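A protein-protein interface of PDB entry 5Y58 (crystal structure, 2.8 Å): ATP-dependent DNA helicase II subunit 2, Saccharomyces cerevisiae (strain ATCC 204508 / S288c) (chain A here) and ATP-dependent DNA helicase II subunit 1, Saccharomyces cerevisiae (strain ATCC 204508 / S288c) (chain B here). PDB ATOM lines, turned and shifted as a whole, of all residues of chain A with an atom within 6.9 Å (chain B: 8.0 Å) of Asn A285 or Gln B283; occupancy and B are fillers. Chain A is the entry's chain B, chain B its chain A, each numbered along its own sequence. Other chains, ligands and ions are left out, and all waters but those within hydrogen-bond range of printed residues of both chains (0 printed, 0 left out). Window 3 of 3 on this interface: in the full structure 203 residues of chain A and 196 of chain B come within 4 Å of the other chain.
The guanidinium group (NH1) of Arg A614 sits close to the backbone carbonyl oxygen (O) of Leu B274 (3.3 Å).
The backbone carbonyl oxygen (O) of Ser A311 lies close to the backbone carbonyl oxygen (O) of Val B275, at 3.5 Å.
The guanidinium group (NH2) of Arg B282 is in hydrogen-bond range of the backbone carbonyl oxygen (O) of Gly A615, 3.3 Å away.
The side-chain amide nitrogen of Gln B283 lies within hydrogen-bond range of the backbone carbonyl oxygen of His A284.
The guanidinium group (NH1) of Arg A614 sits close to the backbone NH (N) of Val B275 (3.3 Å).
The side-chain amide nitrogen (NE2) of Gln B283 lies close to the side-chain amide nitrogen (ND2) of Asn A285.
The backbone carbonyl oxygen (O) of Ser A311 lies within hydrogen-bond range of the backbone NH (N) of Glu B277, 3.1 Å away.
O of Ile A283 is in hydrogen-bond range of N of Val A305 (3.1 Å).
The backbone NH (N) of Tyr B276 lies within hydrogen-bond range of the backbone carbonyl oxygen (O) of Gln B283, 2.5 Å away.
N of Ala B285 sits at hydrogen-bond distance from O of Leu B274.
O of Asn A285 sits at hydrogen-bond distance from N of Ile A303.
CG2 of Ile A283 touches CB of Tyr B276, 3.6 Å away.
Gln B283 touches Ile A283 (NE2 to CB, 3.9 Å).
Ile A283 touches Glu B284 (CG2 to O, 3.9 Å).
ND1 of His A284 touches CE2 of Tyr B286, at 3.4 Å.
Tyr B276 touches Ser A311 (CE1 to OG, 3.1 Å).
Val B275 touches Val A312 (O to CA, 3.4 Å).
Ala B285 touches Val A312 (CB to CG2, 3.8 Å).
Arg A614 touches Glu B284 (CB to OE1, 3.4 Å).
Asn A285 touches just one residue of chain B: Gln B283.
Of the printed residues of chain B, Ser A311 touches Val B275 (3.5 Å), Tyr B276 (3.1 Å) and Glu B277 (3.1 Å).
Of the printed residues of chain A, Leu B274 touches Arg A614 (3.2 Å).
Of the printed residues of chain A, Tyr B276 touches Ile A283 and Ser A311.
Gln B283 touches just these residues of chain A: Ile A283 (3.9 Å), His A284 (2.7 Å) and Asn A285 (3.4 Å).
The nearest residue of chain B that does not touch Asn A285 is Ile B281 (6.5 Å).
The nearest residue of chain A that does not touch Gln B283 is Arg A614 (4.7 Å).
The nearest printed residue of chain B that does not touch Ile A283 is Ala B285 (4.3 Å).
Printed residues of chain B that touch a printed residue of chain A: Leu B274, Val B275, Tyr B276, Glu B277, Arg B282, Gln B283, Glu B284, Ala B285 and Tyr B286.
Printed residues of chain A that touch a printed residue of chain B: Ile A283, His A284, Asn A285, Ser A311, Val A312, Arg A614 and Gly A615.
Hydrophobic or aromatic side chains of chain A within 4 Å of the printed part of chain B: Ile A283, His A284 and Val A312.
Among the printed residues, 15 pairs touch across the chains.
Among the printed residues, no Asp or Glu carboxylate lies within 4 Å of a Lys or Arg side-chain nitrogen of the other chain.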
ATOM      1  N   ILE A 283      14.893  -6.340  -5.259  1.00  0.00           N
ATOM      2  CA  ILE A 283      14.558  -7.463  -4.394  1.00  0.00           C
ATOM      3  C   ILE A 283      14.060  -8.618  -5.249  1.00  0.00           C
ATOM      4  O   ILE A 283      13.614  -8.415  -6.377  1.00  0.00           O
ATOM      5  CB  ILE A 283      13.493  -7.093  -3.347  1.00  0.00           C
ATOM      6  CG1 ILE A 283      12.173  -6.736  -4.026  1.00  0.00           C
ATOM      7  CG2 ILE A 283      13.976  -5.948  -2.482  1.00  0.00           C
ATOM      8  CD1 ILE A 283      11.070  -6.362  -3.055  1.00  0.00           C
ATOM      9  N   HIS A 284      14.138  -9.829  -4.709  1.00  0.00           N
ATOM     10  CA  HIS A 284      13.748 -11.021  -5.452  1.00  0.00           C
ATOM     11  C   HIS A 284      12.490 -11.663  -4.885  1.00  0.00           C
ATOM     12  O   HIS A 284      12.483 -12.147  -3.752  1.00  0.00           O
ATOM     13  CB  HIS A 284      14.886 -12.042  -5.461  1.00  0.00           C
ATOM     14  CG  HIS A 284      16.123 -11.563  -6.154  1.00  0.00           C
ATOM     15  ND1 HIS A 284      17.289 -12.295  -6.181  1.00  0.00           N
ATOM     16  CD2 HIS A 284      16.374 -10.425  -6.844  1.00  0.00           C
ATOM     17  CE1 HIS A 284      18.208 -11.628  -6.863  1.00  0.00           C
ATOM     18  NE2 HIS A 284      17.677 -10.493  -7.274  1.00  0.00           N
ATOM     19  N   ASN A 285      11.429 -11.670  -5.683  1.00  0.00           N
ATOM     20  CA  ASN A 285      10.211 -12.378  -5.325  1.00  0.00           C
ATOM     21  C   ASN A 285      10.167 -13.737  -6.018  1.00  0.00           C
ATOM     22  O   ASN A 285       9.820 -13.833  -7.194  1.00  0.00           O
ATOM     23  CB  ASN A 285       8.980 -11.544  -5.683  1.00  0.00           C
ATOM     24  CG  ASN A 285       8.868 -10.285  -4.846  1.00  0.00           C
ATOM     25  OD1 ASN A 285       8.765  -9.177  -5.373  1.00  0.00           O
ATOM     26  ND2 ASN A 285       8.891 -10.450  -3.528  1.00  0.00           N
ATOM     27  N   GLU A 286      10.535 -14.785  -5.285  1.00  0.00           N
ATOM     28  CA  GLU A 286      10.626 -16.122  -5.863  1.00  0.00           C
ATOM     29  C   GLU A 286       9.256 -16.695  -6.194  1.00  0.00           C
ATOM     30  O   GLU A 286       8.281 -16.459  -5.481  1.00  0.00           O
ATOM     31  CB  GLU A 286      11.367 -17.075  -4.920  1.00  0.00           C
ATOM     32  CG  GLU A 286      12.848 -16.773  -4.756  1.00  0.00           C
ATOM     33  CD  GLU A 286      13.168 -16.110  -3.430  1.00  0.00           C
ATOM     34  OE1 GLU A 286      12.264 -16.012  -2.574  1.00  0.00           O
ATOM     35  OE2 GLU A 286      14.329 -15.689  -3.244  1.00  0.00           O
ATOM     36  N   GLY A 287       9.198 -17.455  -7.282  1.00  0.00           N
ATOM     37  CA  GLY A 287       7.962 -18.074  -7.722  1.00  0.00           C
ATOM     38  C   GLY A 287       8.088 -19.577  -7.868  1.00  0.00           C
ATOM     39  O   GLY A 287       7.135 -20.250  -8.255  1.00  0.00           O
ATOM     40  N   SER A 301      12.530 -19.860 -10.369  1.00  0.00           N
ATOM     41  CA  SER A 301      13.360 -18.662 -10.439  1.00  0.00           C
ATOM     42  C   SER A 301      12.666 -17.492  -9.748  1.00  0.00           C
ATOM     43  O   SER A 301      11.511 -17.603  -9.336  1.00  0.00           O
ATOM     44  CB  SER A 301      13.679 -18.312 -11.895  1.00  0.00           C
ATOM     45  OG  SER A 301      12.497 -18.218 -12.672  1.00  0.00           O
ATOM     46  N   TYR A 302      13.370 -16.370  -9.624  1.00  0.00           N
ATOM     47  CA  TYR A 302      12.835 -15.215  -8.907  1.00  0.00           C
ATOM     48  C   TYR A 302      12.408 -14.079  -9.834  1.00  0.00           C
ATOM     49  O   TYR A 302      12.825 -14.014 -10.989  1.00  0.00           O
ATOM     50  CB  TYR A 302      13.860 -14.697  -7.891  1.00  0.00           C
ATOM     51  CG  TYR A 302      15.218 -14.342  -8.469  1.00  0.00           C
ATOM     52  CD1 TYR A 302      15.427 -13.127  -9.113  1.00  0.00           C
ATOM     53  CD2 TYR A 302      16.295 -15.211  -8.347  1.00  0.00           C
ATOM     54  CE1 TYR A 302      16.665 -12.796  -9.634  1.00  0.00           C
ATOM     55  CE2 TYR A 302      17.541 -14.888  -8.863  1.00  0.00           C
ATOM     56  CZ  TYR A 302      17.719 -13.678  -9.504  1.00  0.00           C
ATOM     57  OH  TYR A 302      18.949 -13.348 -10.019  1.00  0.00           O
ATOM     58  N   ILE A 303      11.570 -13.189  -9.311  1.00  0.00           N
ATOM     59  CA  ILE A 303      11.107 -12.025 -10.060  1.00  0.00           C
ATOM     60  C   ILE A 303      11.732 -10.746  -9.503  1.00  0.00           C
ATOM     61  O   ILE A 303      11.302 -10.246  -8.464  1.00  0.00           O
ATOM     62  CB  ILE A 303       9.571 -11.898 -10.020  1.00  0.00           C
ATOM     63  CG1 ILE A 303       8.910 -13.234 -10.375  1.00  0.00           C
ATOM     64  CG2 ILE A 303       9.101 -10.792 -10.954  1.00  0.00           C
ATOM     65  CD1 ILE A 303       7.397 -13.212 -10.272  1.00  0.00           C
ATOM     66  N   PRO A 304      12.754 -10.219 -10.194  1.00  0.00           N
ATOM     67  CA  PRO A 304      13.478  -9.021  -9.751  1.00  0.00           C
ATOM     68  C   PRO A 304      12.662  -7.743  -9.919  1.00  0.00           C
ATOM     69  O   PRO A 304      12.186  -7.461 -11.018  1.00  0.00           O
ATOM     70  CB  PRO A 304      14.711  -8.992 -10.667  1.00  0.00           C
ATOM     71  CG  PRO A 304      14.753 -10.337 -11.338  1.00  0.00           C
ATOM     72  CD  PRO A 304      13.333 -10.778 -11.426  1.00  0.00           C
ATOM     73  N   VAL A 305      12.510  -6.982  -8.839  1.00  0.00           N
ATOM     74  CA  VAL A 305      11.798  -5.708  -8.886  1.00  0.00           C
ATOM     75  C   VAL A 305      12.674  -4.575  -8.360  1.00  0.00           C
ATOM     76  O   VAL A 305      13.158  -4.630  -7.229  1.00  0.00           O
ATOM     77  CB  VAL A 305      10.495  -5.756  -8.069  1.00  0.00           C
ATOM     78  CG1 VAL A 305       9.760  -4.426  -8.160  1.00  0.00           C
ATOM     79  CG2 VAL A 305       9.610  -6.896  -8.551  1.00  0.00           C
ATOM     80  N   SER A 311      14.876   2.690   0.837  1.00  0.00           N
ATOM     81  CA  SER A 311      14.311   1.567   1.568  1.00  0.00           C
ATOM     82  C   SER A 311      15.336   0.451   1.753  1.00  0.00           C
ATOM     83  O   SER A 311      14.987  -0.665   2.138  1.00  0.00           O
ATOM     84  CB  SER A 311      13.074   1.035   0.845  1.00  0.00           C
ATOM     85  OG  SER A 311      13.370   0.757  -0.512  1.00  0.00           O
ATOM     86  N   VAL A 312      16.601   0.762   1.483  1.00  0.00           N
ATOM     87  CA  VAL A 312      17.680  -0.211   1.618  1.00  0.00           C
ATOM     88  C   VAL A 312      18.683   0.203   2.690  1.00  0.00           C
ATOM     89  O   VAL A 312      19.139   1.345   2.728  1.00  0.00           O
ATOM     90  CB  VAL A 312      18.423  -0.418   0.276  1.00  0.00           C
ATOM     91  CG1 VAL A 312      19.816  -0.998   0.506  1.00  0.00           C
ATOM     92  CG2 VAL A 312      17.611  -1.316  -0.638  1.00  0.00           C
ATOM     93  N   ARG A 614      17.642 -14.704   4.040  1.00  0.00           N
ATOM     94  CA  ARG A 614      17.959 -13.757   5.104  1.00  0.00           C
ATOM     95  C   ARG A 614      16.924 -12.652   5.327  1.00  0.00           C
ATOM     96  O   ARG A 614      16.969 -11.605   4.680  1.00  0.00           O
ATOM     97  CB  ARG A 614      19.307 -13.086   4.828  1.00  0.00           C
ATOM     98  CG  ARG A 614      19.737 -12.124   5.910  1.00  0.00           C
ATOM     99  CD  ARG A 614      19.920 -10.727   5.358  1.00  0.00           C
ATOM    100  NE  ARG A 614      19.592  -9.721   6.360  1.00  0.00           N
ATOM    101  CZ  ARG A 614      19.631  -8.412   6.145  1.00  0.00           C
ATOM    102  NH1 ARG A 614      20.004  -7.941   4.962  1.00  0.00           N
ATOM    103  NH2 ARG A 614      19.306  -7.572   7.119  1.00  0.00           N
ATOM    104  N   GLY A 615      15.993 -12.897   6.246  1.00  0.00           N
ATOM    105  CA  GLY A 615      14.964 -11.927   6.579  1.00  0.00           C
ATOM    106  C   GLY A 615      14.602 -11.960   8.052  1.00  0.00           C
ATOM    107  O   GLY A 615      13.902 -11.079   8.555  1.00  0.00           O
ATOM    108  N   LEU B 274      22.259  -6.692   2.341  1.00  0.00           N
ATOM    109  CA  LEU B 274      21.391  -5.533   2.173  1.00  0.00           C
ATOM    110  C   LEU B 274      19.942  -5.903   2.457  1.00  0.00           C
ATOM    111  O   LEU B 274      19.427  -6.875   1.906  1.00  0.00           O
ATOM    112  CB  LEU B 274      21.528  -4.959   0.760  1.00  0.00           C
ATOM    113  CG  LEU B 274      22.924  -4.492   0.344  1.00  0.00           C
ATOM    114  CD1 LEU B 274      22.897  -3.845  -1.034  1.00  0.00           C
ATOM    115  CD2 LEU B 274      23.492  -3.538   1.381  1.00  0.00           C
ATOM    116  N   VAL B 275      19.289  -5.126   3.317  1.00  0.00           N
ATOM    117  CA  VAL B 275      17.897  -5.386   3.665  1.00  0.00           C
ATOM    118  C   VAL B 275      16.958  -4.307   3.127  1.00  0.00           C
ATOM    119  O   VAL B 275      17.213  -3.111   3.271  1.00  0.00           O
ATOM    120  CB  VAL B 275      17.708  -5.501   5.197  1.00  0.00           C
ATOM    121  CG1 VAL B 275      18.398  -4.354   5.918  1.00  0.00           C
ATOM    122  CG2 VAL B 275      16.228  -5.555   5.562  1.00  0.00           C
ATOM    123  N   TYR B 276      15.875  -4.747   2.498  1.00  0.00           N
ATOM    124  CA  TYR B 276      14.830  -3.851   2.026  1.00  0.00           C
ATOM    125  C   TYR B 276      13.623  -3.949   2.947  1.00  0.00           C
ATOM    126  O   TYR B 276      13.012  -5.011   3.066  1.00  0.00           O
ATOM    127  CB  TYR B 276      14.447  -4.191   0.581  1.00  0.00           C
ATOM    128  CG  TYR B 276      13.106  -3.658   0.130  1.00  0.00           C
ATOM    129  CD1 TYR B 276      12.979  -2.363  -0.353  1.00  0.00           C
ATOM    130  CD2 TYR B 276      11.969  -4.457   0.169  1.00  0.00           C
ATOM    131  CE1 TYR B 276      11.753  -1.875  -0.770  1.00  0.00           C
ATOM    132  CE2 TYR B 276      10.742  -3.977  -0.243  1.00  0.00           C
ATOM    133  CZ  TYR B 276      10.640  -2.685  -0.713  1.00  0.00           C
ATOM    134  OH  TYR B 276       9.421  -2.202  -1.127  1.00  0.00           O
ATOM    135  N   GLU B 277      13.292  -2.849   3.615  1.00  0.00           N
ATOM    136  CA  GLU B 277      12.105  -2.822   4.459  1.00  0.00           C
ATOM    137  C   GLU B 277      11.130  -1.752   3.999  1.00  0.00           C
ATOM    138  O   GLU B 277      11.488  -0.583   3.859  1.00  0.00           O
ATOM    139  CB  GLU B 277      12.468  -2.603   5.928  1.00  0.00           C
ATOM    140  CG  GLU B 277      11.265  -2.727   6.856  1.00  0.00           C
ATOM    141  CD  GLU B 277      11.654  -2.906   8.312  1.00  0.00           C
ATOM    142  OE1 GLU B 277      12.868  -2.909   8.605  1.00  0.00           O
ATOM    143  OE2 GLU B 277      10.747  -3.051   9.160  1.00  0.00           O
ATOM    144  N   HIS B 278       9.894  -2.174   3.756  1.00  0.00           N
ATOM    145  CA  HIS B 278       8.820  -1.279   3.348  1.00  0.00           C
ATOM    146  C   HIS B 278       7.526  -1.710   4.029  1.00  0.00           C
ATOM    147  O   HIS B 278       6.911  -2.705   3.642  1.00  0.00           O
ATOM    148  CB  HIS B 278       8.664  -1.281   1.826  1.00  0.00           C
ATOM    149  CG  HIS B 278       7.728  -0.233   1.311  1.00  0.00           C
ATOM    150  ND1 HIS B 278       7.925   1.113   1.526  1.00  0.00           N
ATOM    151  CD2 HIS B 278       6.587  -0.335   0.586  1.00  0.00           C
ATOM    152  CE1 HIS B 278       6.947   1.797   0.958  1.00  0.00           C
ATOM    153  NE2 HIS B 278       6.124   0.942   0.380  1.00  0.00           N
ATOM    154  N   ASP B 280       5.403  -3.640   6.204  1.00  0.00           N
ATOM    155  CA  ASP B 280       5.455  -4.956   6.834  1.00  0.00           C
ATOM    156  C   ASP B 280       6.267  -5.953   6.008  1.00  0.00           C
ATOM    157  O   ASP B 280       6.195  -7.163   6.228  1.00  0.00           O
ATOM    158  CB  ASP B 280       4.038  -5.491   7.071  1.00  0.00           C
ATOM    159  CG  ASP B 280       3.234  -5.620   5.790  1.00  0.00           C
ATOM    160  OD1 ASP B 280       3.626  -5.008   4.774  1.00  0.00           O
ATOM    161  OD2 ASP B 280       2.205  -6.329   5.806  1.00  0.00           O
ATOM    162  N   ILE B 281       7.045  -5.436   5.063  1.00  0.00           N
ATOM    163  CA  ILE B 281       7.919  -6.273   4.251  1.00  0.00           C
ATOM    164  C   ILE B 281       9.377  -6.099   4.660  1.00  0.00           C
ATOM    165  O   ILE B 281       9.923  -5.004   4.561  1.00  0.00           O
ATOM    166  CB  ILE B 281       7.786  -5.950   2.748  1.00  0.00           C
ATOM    167  CG1 ILE B 281       6.333  -6.092   2.289  1.00  0.00           C
ATOM    168  CG2 ILE B 281       8.698  -6.853   1.924  1.00  0.00           C
ATOM    169  CD1 ILE B 281       5.817  -7.515   2.308  1.00  0.00           C
ATOM    170  N   ARG B 282      10.006  -7.172   5.129  1.00  0.00           N
ATOM    171  CA  ARG B 282      11.442  -7.147   5.379  1.00  0.00           C
ATOM    172  C   ARG B 282      12.109  -8.241   4.549  1.00  0.00           C
ATOM    173  O   ARG B 282      11.855  -9.431   4.743  1.00  0.00           O
ATOM    174  CB  ARG B 282      11.750  -7.312   6.867  1.00  0.00           C
ATOM    175  CG  ARG B 282      13.125  -6.786   7.251  1.00  0.00           C
ATOM    176  CD  ARG B 282      13.286  -6.622   8.754  1.00  0.00           C
ATOM    177  NE  ARG B 282      13.495  -7.896   9.436  1.00  0.00           N
ATOM    178  CZ  ARG B 282      13.774  -8.012  10.730  1.00  0.00           C
ATOM    179  NH1 ARG B 282      13.878  -6.927  11.489  1.00  0.00           N
ATOM    180  NH2 ARG B 282      13.949  -9.213  11.267  1.00  0.00           N
ATOM    181  N   GLN B 283      12.959  -7.822   3.616  1.00  0.00           N
ATOM    182  CA  GLN B 283      13.452  -8.711   2.571  1.00  0.00           C
ATOM    183  C   GLN B 283      14.857  -8.325   2.115  1.00  0.00           C
ATOM    184  O   GLN B 283      15.205  -7.146   2.093  1.00  0.00           O
ATOM    185  CB  GLN B 283      12.480  -8.687   1.389  1.00  0.00           C
ATOM    186  CG  GLN B 283      12.705  -9.755   0.338  1.00  0.00           C
ATOM    187  CD  GLN B 283      11.567  -9.811  -0.668  1.00  0.00           C
ATOM    188  OE1 GLN B 283      10.443  -9.400  -0.374  1.00  0.00           O
ATOM    189  NE2 GLN B 283      11.855 -10.321  -1.859  1.00  0.00           N
ATOM    190  N   GLU B 284      15.659  -9.319   1.748  1.00  0.00           N
ATOM    191  CA  GLU B 284      17.026  -9.071   1.305  1.00  0.00           C
ATOM    192  C   GLU B 284      17.056  -8.308  -0.014  1.00  0.00           C
ATOM    193  O   GLU B 284      16.294  -8.608  -0.934  1.00  0.00           O
ATOM    194  CB  GLU B 284      17.800 -10.386   1.162  1.00  0.00           C
ATOM    195  CG  GLU B 284      19.146 -10.230   0.461  1.00  0.00           C
ATOM    196  CD  GLU B 284      20.142 -11.309   0.838  1.00  0.00           C
ATOM    197  OE1 GLU B 284      19.758 -12.251   1.562  1.00  0.00           O
ATOM    198  OE2 GLU B 284      21.313 -11.211   0.415  1.00  0.00           O
ATOM    199  N   ALA B 285      17.943  -7.321  -0.095  1.00  0.00           N
ATOM    200  CA  ALA B 285      18.112  -6.525  -1.308  1.00  0.00           C
ATOM    201  C   ALA B 285      19.471  -6.778  -1.960  1.00  0.00           C
ATOM    202  O   ALA B 285      20.383  -7.324  -1.332  1.00  0.00           O
ATOM    203  CB  ALA B 285      17.938  -5.047  -0.998  1.00  0.00           C
ATOM    204  N   TYR B 286      19.599  -6.383  -3.225  1.00  0.00           N
ATOM    205  CA  TYR B 286      20.819  -6.632  -3.990  1.00  0.00           C
ATOM    206  C   TYR B 286      21.246  -5.403  -4.788  1.00  0.00           C
ATOM    207  O   TYR B 286      20.406  -4.622  -5.242  1.00  0.00           O
ATOM    208  CB  TYR B 286      20.624  -7.823  -4.935  1.00  0.00           C
ATOM    209  CG  TYR B 286      20.179  -9.086  -4.233  1.00  0.00           C
ATOM    210  CD1 TYR B 286      21.107  -9.977  -3.706  1.00  0.00           C
ATOM    211  CD2 TYR B 286      18.829  -9.385  -4.091  1.00  0.00           C
ATOM    212  CE1 TYR B 286      20.702 -11.132  -3.058  1.00  0.00           C
ATOM    213  CE2 TYR B 286      18.415 -10.534  -3.444  1.00  0.00           C
ATOM    214  CZ  TYR B 286      19.356 -11.404  -2.929  1.00  0.00           C
ATOM    215  OH  TYR B 286      18.951 -12.551  -2.285  1.00  0.00           O
